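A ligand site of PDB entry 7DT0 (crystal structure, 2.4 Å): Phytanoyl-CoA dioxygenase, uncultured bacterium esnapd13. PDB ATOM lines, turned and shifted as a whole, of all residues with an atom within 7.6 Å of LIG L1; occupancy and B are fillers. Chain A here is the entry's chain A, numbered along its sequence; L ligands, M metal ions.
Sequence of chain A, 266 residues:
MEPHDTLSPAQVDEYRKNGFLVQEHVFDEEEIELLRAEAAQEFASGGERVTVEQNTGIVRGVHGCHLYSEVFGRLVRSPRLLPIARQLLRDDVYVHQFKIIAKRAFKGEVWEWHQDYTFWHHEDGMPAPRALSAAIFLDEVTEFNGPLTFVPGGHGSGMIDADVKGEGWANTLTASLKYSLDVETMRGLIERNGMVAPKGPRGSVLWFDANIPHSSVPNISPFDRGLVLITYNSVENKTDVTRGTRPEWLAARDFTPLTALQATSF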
ATOM      1  N   HIS A  63      21.121   9.745  -9.745  1.00  0.00           N
ATOM      2  CA  HIS A  63      21.518  11.096 -10.104  1.00  0.00           C
ATOM      3  C   HIS A  63      22.937  11.420  -9.658  1.00  0.00           C
ATOM      4  O   HIS A  63      23.383  11.026  -8.532  1.00  0.00           O
ATOM      5  CB  HIS A  63      20.564  12.090  -9.477  1.00  0.00           C
ATOM      6  CG  HIS A  63      19.141  11.853  -9.868  1.00  0.00           C
ATOM      7  ND1 HIS A  63      18.471  12.677 -10.747  1.00  0.00           N
ATOM      8  CD2 HIS A  63      18.295  10.845  -9.558  1.00  0.00           C
ATOM      9  CE1 HIS A  63      17.259  12.204 -10.928  1.00  0.00           C
ATOM     10  NE2 HIS A  63      17.134  11.090 -10.227  1.00  0.00           N
ATOM     11  N   HIS A  96      24.953  20.460 -15.781  1.00  0.00           N
ATOM     12  CA  HIS A  96      23.892  20.876 -14.833  1.00  0.00           C
ATOM     13  C   HIS A  96      23.354  19.693 -14.036  1.00  0.00           C
ATOM     14  O   HIS A  96      23.179  19.815 -12.810  1.00  0.00           O
ATOM     15  CB  HIS A  96      22.707  21.533 -15.524  1.00  0.00           C
ATOM     16  CG  HIS A  96      21.594  21.914 -14.613  1.00  0.00           C
ATOM     17  ND1 HIS A  96      21.677  22.959 -13.725  1.00  0.00           N
ATOM     18  CD2 HIS A  96      20.316  21.452 -14.520  1.00  0.00           C
ATOM     19  CE1 HIS A  96      20.538  23.076 -13.067  1.00  0.00           C
ATOM     20  NE2 HIS A  96      19.685  22.184 -13.547  1.00  0.00           N
ATOM     21  N   GLN A  97      23.079  18.584 -14.718  1.00  0.00           N
ATOM     22  CA  GLN A  97      22.593  17.388 -14.046  1.00  0.00           C
ATOM     23  C   GLN A  97      22.950  16.196 -14.866  1.00  0.00           C
ATOM     24  O   GLN A  97      23.180  16.312 -16.086  1.00  0.00           O
ATOM     25  CB  GLN A  97      21.081  17.437 -13.753  1.00  0.00           C
ATOM     26  CG  GLN A  97      20.125  17.157 -14.886  1.00  0.00           C
ATOM     27  CD  GLN A  97      20.145  15.675 -15.306  1.00  0.00           C
ATOM     28  OE1 GLN A  97      20.154  14.778 -14.456  1.00  0.00           O
ATOM     29  NE2 GLN A  97      20.213  15.416 -16.631  1.00  0.00           N
ATOM     30  N   LYS A  99      21.767  12.000 -15.096  1.00  0.00           N
ATOM     31  CA  LYS A  99      21.135  10.831 -14.546  1.00  0.00           C
ATOM     32  C   LYS A  99      21.223   9.601 -15.400  1.00  0.00           C
ATOM     33  O   LYS A  99      21.508   9.679 -16.588  1.00  0.00           O
ATOM     34  CB  LYS A  99      19.717  11.111 -14.152  1.00  0.00           C
ATOM     35  CG  LYS A  99      18.877  11.734 -15.204  1.00  0.00           C
ATOM     36  CD  LYS A  99      17.463  11.846 -14.643  1.00  0.00           C
ATOM     37  CE  LYS A  99      16.565  12.815 -15.398  1.00  0.00           C
ATOM     38  NZ  LYS A  99      15.142  12.727 -14.907  1.00  0.00           N
ATOM     39  N   HIS A 114       6.272  18.149 -20.968  1.00  0.00           N
ATOM     40  CA  HIS A 114       6.926  19.216 -20.235  1.00  0.00           C
ATOM     41  C   HIS A 114       8.078  19.806 -21.011  1.00  0.00           C
ATOM     42  O   HIS A 114       8.569  19.224 -21.969  1.00  0.00           O
ATOM     43  CB  HIS A 114       7.408  18.704 -18.861  1.00  0.00           C
ATOM     44  CG  HIS A 114       8.452  17.634 -18.958  1.00  0.00           C
ATOM     45  ND1 HIS A 114       8.147  16.329 -19.285  1.00  0.00           N
ATOM     46  CD2 HIS A 114       9.793  17.676 -18.761  1.00  0.00           C
ATOM     47  CE1 HIS A 114       9.260  15.611 -19.272  1.00  0.00           C
ATOM     48  NE2 HIS A 114      10.278  16.409 -18.955  1.00  0.00           N
ATOM     49  N   GLN A 115       8.476  20.990 -20.588  1.00  0.00           N
ATOM     50  CA  GLN A 115       9.742  21.561 -20.983  1.00  0.00           C
ATOM     51  C   GLN A 115      10.738  21.502 -19.818  1.00  0.00           C
ATOM     52  O   GLN A 115      10.445  22.033 -18.779  1.00  0.00           O
ATOM     53  CB  GLN A 115       9.501  22.976 -21.388  1.00  0.00           C
ATOM     54  CG  GLN A 115       8.689  23.102 -22.681  1.00  0.00           C
ATOM     55  CD  GLN A 115       8.183  24.517 -22.841  1.00  0.00           C
ATOM     56  OE1 GLN A 115       7.321  24.958 -22.079  1.00  0.00           O
ATOM     57  NE2 GLN A 115       8.752  25.250 -23.773  1.00  0.00           N
ATOM     58  N   ASP A 116      11.906  20.881 -19.996  1.00  0.00           N
ATOM     59  CA  ASP A 116      12.880  20.729 -18.906  1.00  0.00           C
ATOM     60  C   ASP A 116      13.279  22.100 -18.290  1.00  0.00           C
ATOM     61  O   ASP A 116      13.430  22.254 -17.053  1.00  0.00           O
ATOM     62  CB  ASP A 116      14.112  19.961 -19.336  1.00  0.00           C
ATOM     63  CG  ASP A 116      13.837  18.487 -19.601  1.00  0.00           C
ATOM     64  OD1 ASP A 116      12.747  17.987 -19.346  1.00  0.00           O
ATOM     65  OD2 ASP A 116      14.728  17.823 -20.124  1.00  0.00           O
ATOM     66  N   TYR A 117      13.415  23.094 -19.156  1.00  0.00           N
ATOM     67  CA  TYR A 117      13.891  24.368 -18.724  1.00  0.00           C
ATOM     68  C   TYR A 117      12.956  24.979 -17.716  1.00  0.00           C
ATOM     69  O   TYR A 117      13.405  25.699 -16.826  1.00  0.00           O
ATOM     70  CB  TYR A 117      14.079  25.336 -19.885  1.00  0.00           C
ATOM     71  CG  TYR A 117      14.141  26.760 -19.459  1.00  0.00           C
ATOM     72  CD1 TYR A 117      15.295  27.248 -18.868  1.00  0.00           C
ATOM     73  CD2 TYR A 117      13.070  27.624 -19.657  1.00  0.00           C
ATOM     74  CE1 TYR A 117      15.404  28.559 -18.497  1.00  0.00           C
ATOM     75  CE2 TYR A 117      13.165  28.950 -19.272  1.00  0.00           C
ATOM     76  CZ  TYR A 117      14.348  29.407 -18.676  1.00  0.00           C
ATOM     77  OH  TYR A 117      14.554  30.707 -18.275  1.00  0.00           O
ATOM     78  N   THR A 118      11.678  24.731 -17.858  1.00  0.00           N
ATOM     79  CA  THR A 118      10.722  25.361 -16.935  1.00  0.00           C
ATOM     80  C   THR A 118      11.070  24.974 -15.445  1.00  0.00           C
ATOM     81  O   THR A 118      11.140  25.797 -14.570  1.00  0.00           O
ATOM     82  CB  THR A 118       9.254  25.000 -17.384  1.00  0.00           C
ATOM     83  OG1 THR A 118       8.971  25.665 -18.619  1.00  0.00           O
ATOM     84  CG2 THR A 118       8.197  25.446 -16.370  1.00  0.00           C
ATOM     85  N   PHE A 119      11.297  23.703 -15.206  1.00  0.00           N
ATOM     86  CA  PHE A 119      11.673  23.184 -13.904  1.00  0.00           C
ATOM     87  C   PHE A 119      12.981  23.837 -13.455  1.00  0.00           C
ATOM     88  O   PHE A 119      13.073  24.276 -12.340  1.00  0.00           O
ATOM     89  CB  PHE A 119      11.848  21.687 -14.029  1.00  0.00           C
ATOM     90  CG  PHE A 119      11.944  20.961 -12.741  1.00  0.00           C
ATOM     91  CD1 PHE A 119      13.011  21.170 -11.851  1.00  0.00           C
ATOM     92  CD2 PHE A 119      11.022  19.955 -12.458  1.00  0.00           C
ATOM     93  CE1 PHE A 119      13.113  20.433 -10.676  1.00  0.00           C
ATOM     94  CE2 PHE A 119      11.135  19.217 -11.281  1.00  0.00           C
ATOM     95  CZ  PHE A 119      12.179  19.454 -10.385  1.00  0.00           C
ATOM     96  N   TRP A 120      13.964  23.913 -14.338  1.00  0.00           N
ATOM     97  CA  TRP A 120      15.255  24.436 -13.977  1.00  0.00           C
ATOM     98  C   TRP A 120      15.234  25.892 -13.634  1.00  0.00           C
ATOM     99  O   TRP A 120      15.996  26.372 -12.786  1.00  0.00           O
ATOM    100  CB  TRP A 120      16.263  24.131 -15.101  1.00  0.00           C
ATOM    101  CG  TRP A 120      16.541  22.661 -15.269  1.00  0.00           C
ATOM    102  CD1 TRP A 120      16.463  21.704 -14.309  1.00  0.00           C
ATOM    103  CD2 TRP A 120      16.892  21.980 -16.496  1.00  0.00           C
ATOM    104  NE1 TRP A 120      16.795  20.460 -14.848  1.00  0.00           N
ATOM    105  CE2 TRP A 120      17.044  20.603 -16.195  1.00  0.00           C
ATOM    106  CE3 TRP A 120      17.152  22.417 -17.824  1.00  0.00           C
ATOM    107  CZ2 TRP A 120      17.455  19.673 -17.131  1.00  0.00           C
ATOM    108  CZ3 TRP A 120      17.508  21.471 -18.791  1.00  0.00           C
ATOM    109  CH2 TRP A 120      17.650  20.121 -18.449  1.00  0.00           C
ATOM    110  N   GLU A 123      13.182  26.076  -9.966  1.00  0.00           N
ATOM    111  CA  GLU A 123      13.808  25.373  -8.875  1.00  0.00           C
ATOM    112  C   GLU A 123      15.299  25.608  -8.721  1.00  0.00           C
ATOM    113  O   GLU A 123      15.786  25.438  -7.609  1.00  0.00           O
ATOM    114  CB  GLU A 123      13.590  23.887  -9.032  1.00  0.00           C
ATOM    115  CG  GLU A 123      12.146  23.538  -9.329  1.00  0.00           C
ATOM    116  CD  GLU A 123      11.346  23.168  -8.111  1.00  0.00           C
ATOM    117  OE1 GLU A 123      10.621  24.076  -7.619  1.00  0.00           O
ATOM    118  OE2 GLU A 123      11.473  21.966  -7.682  1.00  0.00           O
ATOM    119  N   ASP A 124      16.032  25.874  -9.820  1.00  0.00           N
ATOM    120  CA  ASP A 124      17.520  25.946  -9.807  1.00  0.00           C
ATOM    121  C   ASP A 124      18.071  27.314 -10.167  1.00  0.00           C
ATOM    122  O   ASP A 124      19.262  27.494 -10.128  1.00  0.00           O
ATOM    123  CB  ASP A 124      18.154  24.932 -10.769  1.00  0.00           C
ATOM    124  CG  ASP A 124      17.759  23.496 -10.498  1.00  0.00           C
ATOM    125  OD1 ASP A 124      17.571  23.076  -9.343  1.00  0.00           O
ATOM    126  OD2 ASP A 124      17.654  22.755 -11.492  1.00  0.00           O
ATOM    127  N   ALA A 175       5.269  14.133  -8.742  1.00  0.00           N
ATOM    128  CA  ALA A 175       6.377  13.986  -9.738  1.00  0.00           C
ATOM    129  C   ALA A 175       5.902  13.955 -11.178  1.00  0.00           C
ATOM    130  O   ALA A 175       6.354  14.758 -12.012  1.00  0.00           O
ATOM    131  CB  ALA A 175       7.237  12.763  -9.443  1.00  0.00           C
ATOM    132  N   LYS A 178       4.237  17.856 -11.870  1.00  0.00           N
ATOM    133  CA  LYS A 178       4.951  19.107 -11.655  1.00  0.00           C
ATOM    134  C   LYS A 178       4.723  20.402 -12.489  1.00  0.00           C
ATOM    135  O   LYS A 178       3.863  21.200 -12.148  1.00  0.00           O
ATOM    136  CB  LYS A 178       6.425  18.797 -11.597  1.00  0.00           C
ATOM    137  CG  LYS A 178       6.900  18.440 -10.209  1.00  0.00           C
ATOM    138  CD  LYS A 178       7.875  19.475  -9.733  1.00  0.00           C
ATOM    139  CE  LYS A 178       8.887  18.871  -8.799  1.00  0.00           C
ATOM    140  NZ  LYS A 178       9.309  19.851  -7.780  1.00  0.00           N
ATOM    141  N   TYR A 179       5.521  20.648 -13.514  1.00  0.00           N
ATOM    142  CA  TYR A 179       5.407  21.858 -14.343  1.00  0.00           C
ATOM    143  C   TYR A 179       5.069  21.367 -15.711  1.00  0.00           C
ATOM    144  O   TYR A 179       5.805  21.520 -16.644  1.00  0.00           O
ATOM    145  CB  TYR A 179       6.757  22.583 -14.372  1.00  0.00           C
ATOM    146  CG  TYR A 179       7.227  23.061 -13.077  1.00  0.00           C
ATOM    147  CD1 TYR A 179       7.692  22.188 -12.156  1.00  0.00           C
ATOM    148  CD2 TYR A 179       7.205  24.388 -12.763  1.00  0.00           C
ATOM    149  CE1 TYR A 179       8.106  22.619 -10.925  1.00  0.00           C
ATOM    150  CE2 TYR A 179       7.621  24.846 -11.543  1.00  0.00           C
ATOM    151  CZ  TYR A 179       8.070  23.944 -10.637  1.00  0.00           C
ATOM    152  OH  TYR A 179       8.503  24.331  -9.397  1.00  0.00           O
ATOM    153  N   HIS A 214       8.357  17.704 -24.499  1.00  0.00           N
ATOM    154  CA  HIS A 214       8.433  16.273 -24.687  1.00  0.00           C
ATOM    155  C   HIS A 214       7.793  15.459 -23.583  1.00  0.00           C
ATOM    156  O   HIS A 214       7.485  15.970 -22.522  1.00  0.00           O
ATOM    157  CB  HIS A 214       9.896  15.848 -24.786  1.00  0.00           C
ATOM    158  CG  HIS A 214      10.709  16.204 -23.580  1.00  0.00           C
ATOM    159  ND1 HIS A 214      11.139  17.490 -23.341  1.00  0.00           N
ATOM    160  CD2 HIS A 214      11.140  15.461 -22.528  1.00  0.00           C
ATOM    161  CE1 HIS A 214      11.823  17.519 -22.215  1.00  0.00           C
ATOM    162  NE2 HIS A 214      11.865  16.297 -21.726  1.00  0.00           N
ATOM    163  N   LEU A 229      21.458  10.250 -19.287  1.00  0.00           N
ATOM    164  CA  LEU A 229      21.070  11.579 -19.673  1.00  0.00           C
ATOM    165  C   LEU A 229      21.966  12.669 -19.050  1.00  0.00           C
ATOM    166  O   LEU A 229      22.052  12.816 -17.842  1.00  0.00           O
ATOM    167  CB  LEU A 229      19.622  11.791 -19.280  1.00  0.00           C
ATOM    168  CG  LEU A 229      19.052  13.017 -19.967  1.00  0.00           C
ATOM    169  CD1 LEU A 229      18.362  12.546 -21.201  1.00  0.00           C
ATOM    170  CD2 LEU A 229      18.056  13.771 -19.104  1.00  0.00           C
ATOM    171  N   THR A 231      22.819  16.676 -18.927  1.00  0.00           N
ATOM    172  CA  THR A 231      22.453  18.021 -19.235  1.00  0.00           C
ATOM    173  C   THR A 231      23.617  18.947 -19.108  1.00  0.00           C
ATOM    174  O   THR A 231      24.129  19.149 -18.010  1.00  0.00           O
ATOM    175  CB  THR A 231      21.338  18.532 -18.329  1.00  0.00           C
ATOM    176  OG1 THR A 231      20.181  17.706 -18.492  1.00  0.00           O
ATOM    177  CG2 THR A 231      20.958  19.969 -18.715  1.00  0.00           C
ATOM    178  N   ARG A 246      18.187  22.931  -4.677  1.00  0.00           N
ATOM    179  CA  ARG A 246      18.433  21.474  -4.715  1.00  0.00           C
ATOM    180  C   ARG A 246      19.873  21.179  -4.472  1.00  0.00           C
ATOM    181  O   ARG A 246      20.721  22.052  -4.736  1.00  0.00           O
ATOM    182  CB  ARG A 246      17.951  20.885  -6.034  1.00  0.00           C
ATOM    183  CG  ARG A 246      16.431  21.113  -6.233  1.00  0.00           C
ATOM    184  CD  ARG A 246      15.850  20.220  -7.332  1.00  0.00           C
ATOM    185  NE  ARG A 246      16.350  20.517  -8.703  1.00  0.00           N
ATOM    186  CZ  ARG A 246      16.308  19.624  -9.730  1.00  0.00           C
ATOM    187  NH1 ARG A 246      15.791  18.428  -9.570  1.00  0.00           N
ATOM    188  NH2 ARG A 246      16.724  19.957 -10.931  1.00  0.00           N
ATOM    189  N   LEU A 250      21.817  17.015  -8.112  1.00  0.00           N
ATOM    190  CA  LEU A 250      20.671  17.299  -8.972  1.00  0.00           C
ATOM    191  C   LEU A 250      20.827  18.577  -9.733  1.00  0.00           C
ATOM    192  O   LEU A 250      20.306  18.727 -10.828  1.00  0.00           O
ATOM    193  CB  LEU A 250      19.422  17.472  -8.119  1.00  0.00           C
ATOM    194  CG  LEU A 250      18.841  16.219  -7.435  1.00  0.00           C
ATOM    195  CD1 LEU A 250      17.607  16.556  -6.527  1.00  0.00           C
ATOM    196  CD2 LEU A 250      18.459  15.154  -8.445  1.00  0.00           C
ATOM    197  N   ALA A 251      21.502  19.556  -9.162  1.00  0.00           N
ATOM    198  CA  ALA A 251      21.644  20.849  -9.822  1.00  0.00           C
ATOM    199  C   ALA A 251      22.963  21.444  -9.414  1.00  0.00           C
ATOM    200  O   ALA A 251      23.128  21.846  -8.297  1.00  0.00           O
ATOM    201  CB  ALA A 251      20.468  21.750  -9.503  1.00  0.00           C
HETATM  202  N1  LIG L   1      13.073  16.622 -14.267  1.00  0.00           N
HETATM  203  C1  LIG L   1      14.341  17.330 -14.597  1.00  0.00           C
HETATM  204  C2  LIG L   1      15.242  17.567 -13.361  1.00  0.00           C
HETATM  205  O1  LIG L   1      15.007  16.941 -12.331  1.00  0.00           O
HETATM  206  C3  LIG L   1      13.858  18.669 -15.187  1.00  0.00           C
HETATM  207  C4  LIG L   1      12.468  18.386 -15.709  1.00  0.00           C
HETATM  208  C5  LIG L   1      11.918  17.186 -14.987  1.00  0.00           C
HETATM  209  O2  LIG L   1      16.197  18.379 -13.338  1.00  0.00           O
HETATM  210  C1  LG2 L   2      14.133  14.352 -19.144  1.00  0.00           C
HETATM  211  O1  LG2 L   2      14.367  15.321 -19.942  1.00  0.00           O
HETATM  212  O2  LG2 L   2      14.794  14.217 -18.076  1.00  0.00           O
HETATM  213  C2  LG2 L   2      12.980  13.404 -19.353  1.00  0.00           C
HETATM  214  O3  LG2 L   2      11.849  13.822 -19.608  1.00  0.00           O
HETATM  215  C3  LG2 L   2      13.191  11.935 -19.163  1.00  0.00           C
HETATM  216  C4  LG2 L   2      11.878  11.176 -18.941  1.00  0.00           C
HETATM  217  C5  LG2 L   2      12.131   9.649 -18.960  1.00  0.00           C
HETATM  218  O4  LG2 L   2      11.766   8.942 -17.981  1.00  0.00           O
HETATM  219  O5  LG2 L   2      12.684   9.146 -19.972  1.00  0.00           O
HETATM  220 FE    FE M   1      12.245  16.028 -19.524  1.00  0.00          FE
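The indole nitrogen of Trp 120 sits at hydrogen-bond distance from an oxygen (O2) of LIG L1 (2.6 Å).
NH2 of Arg 246 is in salt-bridge range of O2 of LIG L1 (2.9 Å).
The side-chain amino group of Lys 99 is in salt-bridge range of an oxygen (O2) of LG2 L2 (3.5 Å).
OD1 of Asp 124 is in salt-bridge range of NE of Arg 246, 2.9 Å away.
OD1 of Asp 116 touches C4 of LIG L1 (3.7 Å).
Phe 119 touches LIG L1.
Hydrophobic or aromatic side chains that line LIG L1: Phe 119 and Trp 120.
Four residues have an atom within 4 Å of LIG L1: Asp 116, Phe 119, Trp 120 and Arg 246.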
